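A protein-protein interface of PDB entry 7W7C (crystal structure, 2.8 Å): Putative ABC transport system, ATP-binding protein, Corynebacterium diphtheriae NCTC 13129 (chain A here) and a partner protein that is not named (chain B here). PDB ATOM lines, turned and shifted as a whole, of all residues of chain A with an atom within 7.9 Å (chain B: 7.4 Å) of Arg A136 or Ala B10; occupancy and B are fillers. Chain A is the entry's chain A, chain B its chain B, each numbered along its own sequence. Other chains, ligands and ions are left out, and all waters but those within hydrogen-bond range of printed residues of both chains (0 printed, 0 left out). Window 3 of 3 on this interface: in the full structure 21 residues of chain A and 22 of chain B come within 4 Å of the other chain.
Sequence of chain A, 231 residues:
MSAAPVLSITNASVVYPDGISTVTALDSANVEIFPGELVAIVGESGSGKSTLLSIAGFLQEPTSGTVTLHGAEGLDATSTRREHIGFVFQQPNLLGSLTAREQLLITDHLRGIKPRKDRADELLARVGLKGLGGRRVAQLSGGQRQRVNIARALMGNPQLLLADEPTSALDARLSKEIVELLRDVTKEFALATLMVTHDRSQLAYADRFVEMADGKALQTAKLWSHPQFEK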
ATOM      1  N   LEU A  94      11.435  11.434   3.066  1.00  0.00           N
ATOM      2  CA  LEU A  94      12.151  12.692   3.184  1.00  0.00           C
ATOM      3  C   LEU A  94      11.180  13.799   3.572  1.00  0.00           C
ATOM      4  O   LEU A  94      10.002  13.782   3.200  1.00  0.00           O
ATOM      5  CB  LEU A  94      12.860  13.047   1.876  1.00  0.00           C
ATOM      6  CG  LEU A  94      13.860  12.024   1.331  1.00  0.00           C
ATOM      7  CD1 LEU A  94      14.469  12.504   0.031  1.00  0.00           C
ATOM      8  CD2 LEU A  94      14.945  11.757   2.363  1.00  0.00           C
ATOM      9  N   LEU A  95      11.684  14.764   4.330  1.00  0.00           N
ATOM     10  CA  LEU A  95      10.860  15.841   4.855  1.00  0.00           C
ATOM     11  C   LEU A  95      10.878  17.001   3.866  1.00  0.00           C
ATOM     12  O   LEU A  95      11.947  17.520   3.527  1.00  0.00           O
ATOM     13  CB  LEU A  95      11.363  16.259   6.234  1.00  0.00           C
ATOM     14  CG  LEU A  95      11.477  15.058   7.181  1.00  0.00           C
ATOM     15  CD1 LEU A  95      11.867  15.493   8.593  1.00  0.00           C
ATOM     16  CD2 LEU A  95      10.196  14.213   7.186  1.00  0.00           C
ATOM     17  N   GLY A  96       9.687  17.408   3.415  1.00  0.00           N
ATOM     18  CA  GLY A  96       9.593  18.253   2.235  1.00  0.00           C
ATOM     19  C   GLY A  96      10.253  19.609   2.400  1.00  0.00           C
ATOM     20  O   GLY A  96      10.857  20.134   1.461  1.00  0.00           O
ATOM     21  N   SER A  97      10.155  20.191   3.599  1.00  0.00           N
ATOM     22  CA  SER A  97      10.704  21.526   3.811  1.00  0.00           C
ATOM     23  C   SER A  97      12.225  21.532   3.840  1.00  0.00           C
ATOM     24  O   SER A  97      12.830  22.602   3.721  1.00  0.00           O
ATOM     25  CB  SER A  97      10.159  22.125   5.109  1.00  0.00           C
ATOM     26  OG  SER A  97      10.276  21.216   6.191  1.00  0.00           O
ATOM     27  N   LEU A  98      12.852  20.368   3.977  1.00  0.00           N
ATOM     28  CA  LEU A  98      14.296  20.289   4.103  1.00  0.00           C
ATOM     29  C   LEU A  98      14.949  20.028   2.753  1.00  0.00           C
ATOM     30  O   LEU A  98      14.378  19.375   1.873  1.00  0.00           O
ATOM     31  CB  LEU A  98      14.683  19.189   5.093  1.00  0.00           C
ATOM     32  CG  LEU A  98      14.092  19.335   6.496  1.00  0.00           C
ATOM     33  CD1 LEU A  98      14.465  18.150   7.373  1.00  0.00           C
ATOM     34  CD2 LEU A  98      14.574  20.621   7.118  1.00  0.00           C
ATOM     35  N   THR A  99      16.152  20.570   2.593  1.00  0.00           N
ATOM     36  CA  THR A  99      16.995  20.241   1.456  1.00  0.00           C
ATOM     37  C   THR A  99      17.601  18.854   1.649  1.00  0.00           C
ATOM     38  O   THR A  99      17.564  18.282   2.743  1.00  0.00           O
ATOM     39  CB  THR A  99      18.106  21.281   1.287  1.00  0.00           C
ATOM     40  OG1 THR A  99      18.985  21.232   2.420  1.00  0.00           O
ATOM     41  CG2 THR A  99      17.519  22.682   1.178  1.00  0.00           C
ATOM     42  N   ALA A 100      18.153  18.308   0.561  1.00  0.00           N
ATOM     43  CA  ALA A 100      18.766  16.983   0.627  1.00  0.00           C
ATOM     44  C   ALA A 100      19.798  16.910   1.745  1.00  0.00           C
ATOM     45  O   ALA A 100      19.764  16.003   2.584  1.00  0.00           O
ATOM     46  CB  ALA A 100      19.403  16.631  -0.716  1.00  0.00           C
ATOM     47  N   ARG A 101      20.720  17.875   1.775  1.00  0.00           N
ATOM     48  CA  ARG A 101      21.723  17.929   2.836  1.00  0.00           C
ATOM     49  C   ARG A 101      21.070  18.020   4.211  1.00  0.00           C
ATOM     50  O   ARG A 101      21.550  17.422   5.184  1.00  0.00           O
ATOM     51  CB  ARG A 101      22.648  19.121   2.598  1.00  0.00           C
ATOM     52  CG  ARG A 101      23.946  19.092   3.370  1.00  0.00           C
ATOM     53  CD  ARG A 101      24.665  20.445   3.309  1.00  0.00           C
ATOM     54  NE  ARG A 101      24.937  20.901   1.944  1.00  0.00           N
ATOM     55  CZ  ARG A 101      24.217  21.817   1.302  1.00  0.00           C
ATOM     56  NH1 ARG A 101      23.173  22.380   1.895  1.00  0.00           N
ATOM     57  NH2 ARG A 101      24.536  22.163   0.063  1.00  0.00           N
ATOM     58  N   GLU A 102      19.964  18.758   4.313  1.00  0.00           N
ATOM     59  CA  GLU A 102      19.291  18.895   5.597  1.00  0.00           C
ATOM     60  C   GLU A 102      18.626  17.599   6.046  1.00  0.00           C
ATOM     61  O   GLU A 102      18.491  17.377   7.257  1.00  0.00           O
ATOM     62  CB  GLU A 102      18.274  20.033   5.522  1.00  0.00           C
ATOM     63  CG  GLU A 102      18.907  21.413   5.639  1.00  0.00           C
ATOM     64  CD  GLU A 102      17.965  22.531   5.233  1.00  0.00           C
ATOM     65  OE1 GLU A 102      17.070  22.277   4.397  1.00  0.00           O
ATOM     66  OE2 GLU A 102      18.131  23.663   5.746  1.00  0.00           O
ATOM     67  N   GLN A 103      18.234  16.731   5.103  1.00  0.00           N
ATOM     68  CA  GLN A 103      17.757  15.399   5.469  1.00  0.00           C
ATOM     69  C   GLN A 103      18.800  14.662   6.299  1.00  0.00           C
ATOM     70  O   GLN A 103      18.457  13.937   7.241  1.00  0.00           O
ATOM     71  CB  GLN A 103      17.413  14.587   4.219  1.00  0.00           C
ATOM     72  CG  GLN A 103      16.572  15.314   3.172  1.00  0.00           C
ATOM     73  CD  GLN A 103      15.114  15.450   3.564  1.00  0.00           C
ATOM     74  OE1 GLN A 103      14.634  14.751   4.457  1.00  0.00           O
ATOM     75  NE2 GLN A 103      14.399  16.350   2.897  1.00  0.00           N
ATOM     76  N   LEU A 132      24.626  17.722  -4.908  1.00  0.00           N
ATOM     77  CA  LEU A 132      23.191  17.958  -4.854  1.00  0.00           C
ATOM     78  C   LEU A 132      22.702  18.263  -3.446  1.00  0.00           C
ATOM     79  O   LEU A 132      21.513  18.084  -3.164  1.00  0.00           O
ATOM     80  CB  LEU A 132      22.434  16.760  -5.429  1.00  0.00           C
ATOM     81  CG  LEU A 132      22.617  16.499  -6.926  1.00  0.00           C
ATOM     82  CD1 LEU A 132      21.628  15.450  -7.420  1.00  0.00           C
ATOM     83  CD2 LEU A 132      22.475  17.784  -7.718  1.00  0.00           C
ATOM     84  N   GLY A 133      23.590  18.733  -2.562  1.00  0.00           N
ATOM     85  CA  GLY A 133      23.195  18.977  -1.183  1.00  0.00           C
ATOM     86  C   GLY A 133      22.065  19.979  -1.042  1.00  0.00           C
ATOM     87  O   GLY A 133      21.290  19.915  -0.086  1.00  0.00           O
ATOM     88  N   GLY A 134      21.942  20.900  -1.992  1.00  0.00           N
ATOM     89  CA  GLY A 134      20.942  21.940  -1.921  1.00  0.00           C
ATOM     90  C   GLY A 134      19.619  21.645  -2.593  1.00  0.00           C
ATOM     91  O   GLY A 134      18.683  22.441  -2.451  1.00  0.00           O
ATOM     92  N   ARG A 135      19.505  20.533  -3.318  1.00  0.00           N
ATOM     93  CA  ARG A 135      18.272  20.228  -4.036  1.00  0.00           C
ATOM     94  C   ARG A 135      17.110  20.042  -3.069  1.00  0.00           C
ATOM     95  O   ARG A 135      17.254  19.436  -2.003  1.00  0.00           O
ATOM     96  CB  ARG A 135      18.445  18.966  -4.883  1.00  0.00           C
ATOM     97  CG  ARG A 135      19.391  19.099  -6.067  1.00  0.00           C
ATOM     98  CD  ARG A 135      18.730  19.796  -7.254  1.00  0.00           C
ATOM     99  NE  ARG A 135      19.600  19.811  -8.430  1.00  0.00           N
ATOM    100  CZ  ARG A 135      19.635  18.851  -9.347  1.00  0.00           C
ATOM    101  NH1 ARG A 135      18.840  17.795  -9.221  1.00  0.00           N
ATOM    102  NH2 ARG A 135      20.466  18.952 -10.380  1.00  0.00           N
ATOM    103  N   ARG A 136      15.952  20.582  -3.439  1.00  0.00           N
ATOM    104  CA  ARG A 136      14.734  20.312  -2.694  1.00  0.00           C
ATOM    105  C   ARG A 136      14.166  18.955  -3.103  1.00  0.00           C
ATOM    106  O   ARG A 136      14.501  18.406  -4.155  1.00  0.00           O
ATOM    107  CB  ARG A 136      13.700  21.416  -2.926  1.00  0.00           C
ATOM    108  CG  ARG A 136      13.955  22.706  -2.152  1.00  0.00           C
ATOM    109  CD  ARG A 136      13.528  22.587  -0.695  1.00  0.00           C
ATOM    110  NE  ARG A 136      12.877  23.805  -0.213  1.00  0.00           N
ATOM    111  CZ  ARG A 136      11.559  23.970  -0.150  1.00  0.00           C
ATOM    112  NH1 ARG A 136      10.755  22.990  -0.533  1.00  0.00           N
ATOM    113  NH2 ARG A 136      11.046  25.107   0.299  1.00  0.00           N
ATOM    114  N   VAL A 137      13.295  18.415  -2.247  1.00  0.00           N
ATOM    115  CA  VAL A 137      12.795  17.055  -2.452  1.00  0.00           C
ATOM    116  C   VAL A 137      12.043  16.947  -3.775  1.00  0.00           C
ATOM    117  O   VAL A 137      12.126  15.926  -4.470  1.00  0.00           O
ATOM    118  CB  VAL A 137      11.923  16.625  -1.257  1.00  0.00           C
ATOM    119  CG1 VAL A 137      11.187  15.334  -1.562  1.00  0.00           C
ATOM    120  CG2 VAL A 137      12.779  16.464  -0.011  1.00  0.00           C
ATOM    121  N   ALA A 138      11.321  18.004  -4.158  1.00  0.00           N
ATOM    122  CA  ALA A 138      10.596  17.984  -5.422  1.00  0.00           C
ATOM    123  C   ALA A 138      11.526  17.863  -6.622  1.00  0.00           C
ATOM    124  O   ALA A 138      11.076  17.464  -7.705  1.00  0.00           O
ATOM    125  CB  ALA A 138       9.739  19.245  -5.559  1.00  0.00           C
ATOM    126  N   GLN A 139      12.809  18.187  -6.456  1.00  0.00           N
ATOM    127  CA  GLN A 139      13.768  18.127  -7.549  1.00  0.00           C
ATOM    128  C   GLN A 139      14.511  16.800  -7.631  1.00  0.00           C
ATOM    129  O   GLN A 139      15.286  16.606  -8.571  1.00  0.00           O
ATOM    130  CB  GLN A 139      14.775  19.277  -7.431  1.00  0.00           C
ATOM    131  CG  GLN A 139      14.212  20.628  -7.855  1.00  0.00           C
ATOM    132  CD  GLN A 139      14.151  21.634  -6.713  1.00  0.00           C
ATOM    133  OE1 GLN A 139      15.120  21.816  -5.972  1.00  0.00           O
ATOM    134  NE2 GLN A 139      13.002  22.286  -6.560  1.00  0.00           N
ATOM    135  N   LEU A 140      14.281  15.877  -6.699  1.00  0.00           N
ATOM    136  CA  LEU A 140      14.977  14.597  -6.677  1.00  0.00           C
ATOM    137  C   LEU A 140      14.091  13.502  -7.254  1.00  0.00           C
ATOM    138  O   LEU A 140      12.911  13.401  -6.903  1.00  0.00           O
ATOM    139  CB  LEU A 140      15.396  14.225  -5.253  1.00  0.00           C
ATOM    140  CG  LEU A 140      16.415  15.118  -4.545  1.00  0.00           C
ATOM    141  CD1 LEU A 140      16.718  14.555  -3.161  1.00  0.00           C
ATOM    142  CD2 LEU A 140      17.682  15.243  -5.367  1.00  0.00           C
ATOM    143  N   SER A 141      14.663  12.693  -8.139  1.00  0.00           N
ATOM    144  CA  SER A 141      13.959  11.535  -8.665  1.00  0.00           C
ATOM    145  C   SER A 141      13.905  10.427  -7.611  1.00  0.00           C
ATOM    146  O   SER A 141      14.682  10.408  -6.651  1.00  0.00           O
ATOM    147  CB  SER A 141      14.650  11.024  -9.928  1.00  0.00           C
ATOM    148  OG  SER A 141      15.915  10.455  -9.634  1.00  0.00           O
ATOM    149  N   GLN A 144      17.131   9.058  -6.698  1.00  0.00           N
ATOM    150  CA  GLN A 144      17.925   9.994  -5.905  1.00  0.00           C
ATOM    151  C   GLN A 144      17.370  10.142  -4.497  1.00  0.00           C
ATOM    152  O   GLN A 144      18.132  10.273  -3.529  1.00  0.00           O
ATOM    153  CB  GLN A 144      17.976  11.352  -6.596  1.00  0.00           C
ATOM    154  CG  GLN A 144      18.492  11.259  -8.014  1.00  0.00           C
ATOM    155  CD  GLN A 144      18.691  12.614  -8.659  1.00  0.00           C
ATOM    156  OE1 GLN A 144      17.801  13.465  -8.617  1.00  0.00           O
ATOM    157  NE2 GLN A 144      19.869  12.825  -9.262  1.00  0.00           N
ATOM    158  N   ARG A 145      16.043  10.148  -4.368  1.00  0.00           N
ATOM    159  CA  ARG A 145      15.412  10.153  -3.053  1.00  0.00           C
ATOM    160  C   ARG A 145      15.890   8.975  -2.218  1.00  0.00           C
ATOM    161  O   ARG A 145      16.246   9.130  -1.044  1.00  0.00           O
ATOM    162  CB  ARG A 145      13.895  10.100  -3.200  1.00  0.00           C
ATOM    163  CG  ARG A 145      13.314  11.255  -3.964  1.00  0.00           C
ATOM    164  CD  ARG A 145      12.530  12.174  -3.062  1.00  0.00           C
ATOM    165  NE  ARG A 145      11.646  13.015  -3.853  1.00  0.00           N
ATOM    166  CZ  ARG A 145      10.483  12.608  -4.346  1.00  0.00           C
ATOM    167  NH1 ARG A 145      10.066  11.363  -4.124  1.00  0.00           N
ATOM    168  NH2 ARG A 145       9.746  13.447  -5.063  1.00  0.00           N
ATOM    169  N   GLY B   4      10.993  23.092  12.641  1.00  0.00           N
ATOM    170  CA  GLY B   4       9.988  24.135  12.775  1.00  0.00           C
ATOM    171  C   GLY B   4      10.321  25.369  11.955  1.00  0.00           C
ATOM    172  O   GLY B   4       9.498  25.855  11.172  1.00  0.00           O
ATOM    173  N   ILE B   5      11.544  25.877  12.109  1.00  0.00           N
ATOM    174  CA  ILE B   5      11.960  27.056  11.357  1.00  0.00           C
ATOM    175  C   ILE B   5      11.982  26.757   9.865  1.00  0.00           C
ATOM    176  O   ILE B   5      11.584  27.595   9.041  1.00  0.00           O
ATOM    177  CB  ILE B   5      13.331  27.548  11.856  1.00  0.00           C
ATOM    178  CG1 ILE B   5      13.251  27.944  13.330  1.00  0.00           C
ATOM    179  CG2 ILE B   5      13.817  28.714  11.007  1.00  0.00           C
ATOM    180  CD1 ILE B   5      14.598  28.227  13.956  1.00  0.00           C
ATOM    181  N   ARG B   6      12.450  25.562   9.488  1.00  0.00           N
ATOM    182  CA  ARG B   6      12.474  25.220   8.069  1.00  0.00           C
ATOM    183  C   ARG B   6      11.061  25.144   7.496  1.00  0.00           C
ATOM    184  O   ARG B   6      10.832  25.509   6.339  1.00  0.00           O
ATOM    185  CB  ARG B   6      13.212  23.903   7.852  1.00  0.00           C
ATOM    186  CG  ARG B   6      14.630  23.873   8.398  1.00  0.00           C
ATOM    187  CD  ARG B   6      15.537  24.900   7.761  1.00  0.00           C
ATOM    188  NE  ARG B   6      16.941  24.512   7.899  1.00  0.00           N
ATOM    189  CZ  ARG B   6      17.694  24.782   8.961  1.00  0.00           C
ATOM    190  NH1 ARG B   6      18.962  24.395   8.999  1.00  0.00           N
ATOM    191  NH2 ARG B   6      17.180  25.443   9.988  1.00  0.00           N
ATOM    192  N   ASP B   7      10.103  24.667   8.293  1.00  0.00           N
ATOM    193  CA  ASP B   7       8.704  24.665   7.881  1.00  0.00           C
ATOM    194  C   ASP B   7       8.197  26.084   7.675  1.00  0.00           C
ATOM    195  O   ASP B   7       7.520  26.377   6.683  1.00  0.00           O
ATOM    196  CB  ASP B   7       7.852  23.944   8.929  1.00  0.00           C
ATOM    197  CG  ASP B   7       7.956  22.435   8.836  1.00  0.00           C
ATOM    198  OD1 ASP B   7       8.668  21.932   7.943  1.00  0.00           O
ATOM    199  OD2 ASP B   7       7.318  21.747   9.660  1.00  0.00           O
ATOM    200  N   ILE B   8       8.505  26.976   8.621  1.00  0.00           N
ATOM    201  CA  ILE B   8       8.127  28.383   8.477  1.00  0.00           C
ATOM    202  C   ILE B   8       8.643  28.931   7.153  1.00  0.00           C
ATOM    203  O   ILE B   8       7.919  29.598   6.404  1.00  0.00           O
ATOM    204  CB  ILE B   8       8.660  29.214   9.657  1.00  0.00           C
ATOM    205  CG1 ILE B   8       8.219  28.622  10.997  1.00  0.00           C
ATOM    206  CG2 ILE B   8       8.205  30.662   9.529  1.00  0.00           C
ATOM    207  CD1 ILE B   8       6.733  28.466  11.131  1.00  0.00           C
ATOM    208  N   ARG B   9       9.913  28.650   6.853  1.00  0.00           N
ATOM    209  CA  ARG B   9      10.524  29.150   5.626  1.00  0.00           C
ATOM    210  C   ARG B   9       9.846  28.569   4.389  1.00  0.00           C
ATOM    211  O   ARG B   9       9.434  29.304   3.485  1.00  0.00           O
ATOM    212  CB  ARG B   9      12.017  28.820   5.626  1.00  0.00           C
ATOM    213  CG  ARG B   9      12.768  29.255   4.381  1.00  0.00           C
ATOM    214  CD  ARG B   9      14.164  28.643   4.358  1.00  0.00           C
ATOM    215  NE  ARG B   9      14.106  27.184   4.397  1.00  0.00           N
ATOM    216  CZ  ARG B   9      15.169  26.387   4.442  1.00  0.00           C
ATOM    217  NH1 ARG B   9      16.389  26.905   4.453  1.00  0.00           N
ATOM    218  NH2 ARG B   9      15.011  25.067   4.475  1.00  0.00           N
ATOM    219  N   ALA B  10       9.707  27.241   4.344  1.00  0.00           N
ATOM    220  CA  ALA B  10       9.231  26.577   3.135  1.00  0.00           C
ATOM    221  C   ALA B  10       7.760  26.860   2.863  1.00  0.00           C
ATOM    222  O   ALA B  10       7.347  26.903   1.700  1.00  0.00           O
ATOM    223  CB  ALA B  10       9.473  25.072   3.238  1.00  0.00           C
ATOM    224  N   ALA B  11       6.955  27.048   3.908  1.00  0.00           N
ATOM    225  CA  ALA B  11       5.542  27.355   3.728  1.00  0.00           C
ATOM    226  C   ALA B  11       5.246  28.761   4.229  1.00  0.00           C
ATOM    227  O   ALA B  11       4.373  28.955   5.083  1.00  0.00           O
ATOM    228  CB  ALA B  11       4.668  26.330   4.453  1.00  0.00           C
ATOM    229  N   ALA B  12       5.967  29.747   3.690  1.00  0.00           N
ATOM    230  CA  ALA B  12       5.901  31.101   4.227  1.00  0.00           C
ATOM    231  C   ALA B  12       4.520  31.720   4.057  1.00  0.00           C
ATOM    232  O   ALA B  12       4.136  32.591   4.843  1.00  0.00           O
ATOM    233  CB  ALA B  12       6.965  31.977   3.566  1.00  0.00           C
ATOM    234  N   GLY B  13       3.756  31.280   3.060  1.00  0.00           N
ATOM    235  CA  GLY B  13       2.444  31.847   2.802  1.00  0.00           C
ATOM    236  C   GLY B  13       1.437  31.646   3.917  1.00  0.00           C
ATOM    237  O   GLY B  13       0.878  32.618   4.439  1.00  0.00           O
ATOM    238  N   PHE B  15       1.917  30.617   7.000  1.00  0.00           N
ATOM    239  CA  PHE B  15       2.380  31.162   8.270  1.00  0.00           C
ATOM    240  C   PHE B  15       2.295  32.684   8.284  1.00  0.00           C
ATOM    241  O   PHE B  15       1.955  33.278   9.312  1.00  0.00           O
ATOM    242  CB  PHE B  15       3.802  30.686   8.559  1.00  0.00           C
ATOM    243  CG  PHE B  15       3.880  29.240   8.967  1.00  0.00           C
ATOM    244  CD1 PHE B  15       3.311  28.813  10.157  1.00  0.00           C
ATOM    245  CD2 PHE B  15       4.515  28.309   8.164  1.00  0.00           C
ATOM    246  CE1 PHE B  15       3.375  27.485  10.538  1.00  0.00           C
ATOM    247  CE2 PHE B  15       4.583  26.980   8.541  1.00  0.00           C
ATOM    248  CZ  PHE B  15       4.013  26.570   9.730  1.00  0.00           C
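OD1 of Asp B7 lies within hydrogen-bond range of OG of Ser A97 (2.5 Å).
The side-chain carboxylate (OE2) of Glu A102 is in salt-bridge range of the guanidinium group (NE) of Arg B6 (2.6 Å).
The backbone carbonyl oxygen (O) of Ser A97 sits at hydrogen-bond distance from the guanidinium group (NH2) of Arg B9, 3.4 Å away.
The guanidinium group of Arg B9 is in salt-bridge range of the side-chain carboxylate of Glu A102, at 3.5 Å.
O of Gly A96 lies within hydrogen-bond range of NH1 of Arg A136, at 3.5 Å.
The side-chain amide nitrogen (NE2) of Gln A103 sits at hydrogen-bond distance from the backbone carbonyl oxygen (O) of Leu A98 (3.2 Å).
The backbone NH (N) of Arg A136 is in hydrogen-bond range of the side-chain amide oxygen (OE1) of Gln A139 (2.9 Å).
The backbone NH (N) of Thr A99 lies within hydrogen-bond range of the side-chain carboxylate (OE1) of Glu A102, 2.6 Å away.
Ser A97 touches Arg B6.
Ala B10 touches Ser A97 (CB to CB, 3.6 Å).
CG of Arg B6 touches CD2 of Leu A98 (3.5 Å).
Arg A136 touches Ala B10 (NH2 to CB, 3.3 Å).
Of chain B, only Ala B10 (3.3 Å) comes within 4 Å of Arg A136.
Of the printed residues of chain A, Ala B10 touches Ser A97 (3.6 Å) and Arg A136 (3.3 Å).
Printed residues of chain A within 4 Å of Asp B7: Ser A97.
Printed residues of chain B within 4 Å of Leu A98: Arg B6 (3.5 Å).
Of the printed residues of chain A, Arg B6 touches Ser A97, Leu A98 and Glu A102.
Printed residues of chain B within 4 Å of Ser A97: Arg B6 (3.7 Å), Asp B7 (2.5 Å), Arg B9 (3.4 Å) and Ala B10 (3.6 Å).
Of the printed residues of chain B, Glu A102 touches Arg B6 and Arg B9.
Gly A134 touches none of the printed residues of chain B.
The nearest residue of chain B that does not touch Arg A136 is Arg B9 (5.3 Å).
The nearest printed residue of chain A that does not touch Arg B6 is Arg A136 (6.1 Å).
Along chain B the printed residues that touch a printed residue of chain A span positions 6 to 10.
Of the 22 printed residues of chain A, 4 touch a printed residue of chain B.
Printed residues of chain A that touch a printed residue of chain B: Ser A97, Leu A98, Glu A102 and Arg A136.
Hydrophobic or aromatic side chains of chain A that line the printed part of chain B: Leu A98.
Among the printed residues, Asp or Glu carboxylates within 4 Å of a Lys or Arg side-chain nitrogen of the other chain: Glu A102 with Arg B6 and Glu A102 with Arg B9.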
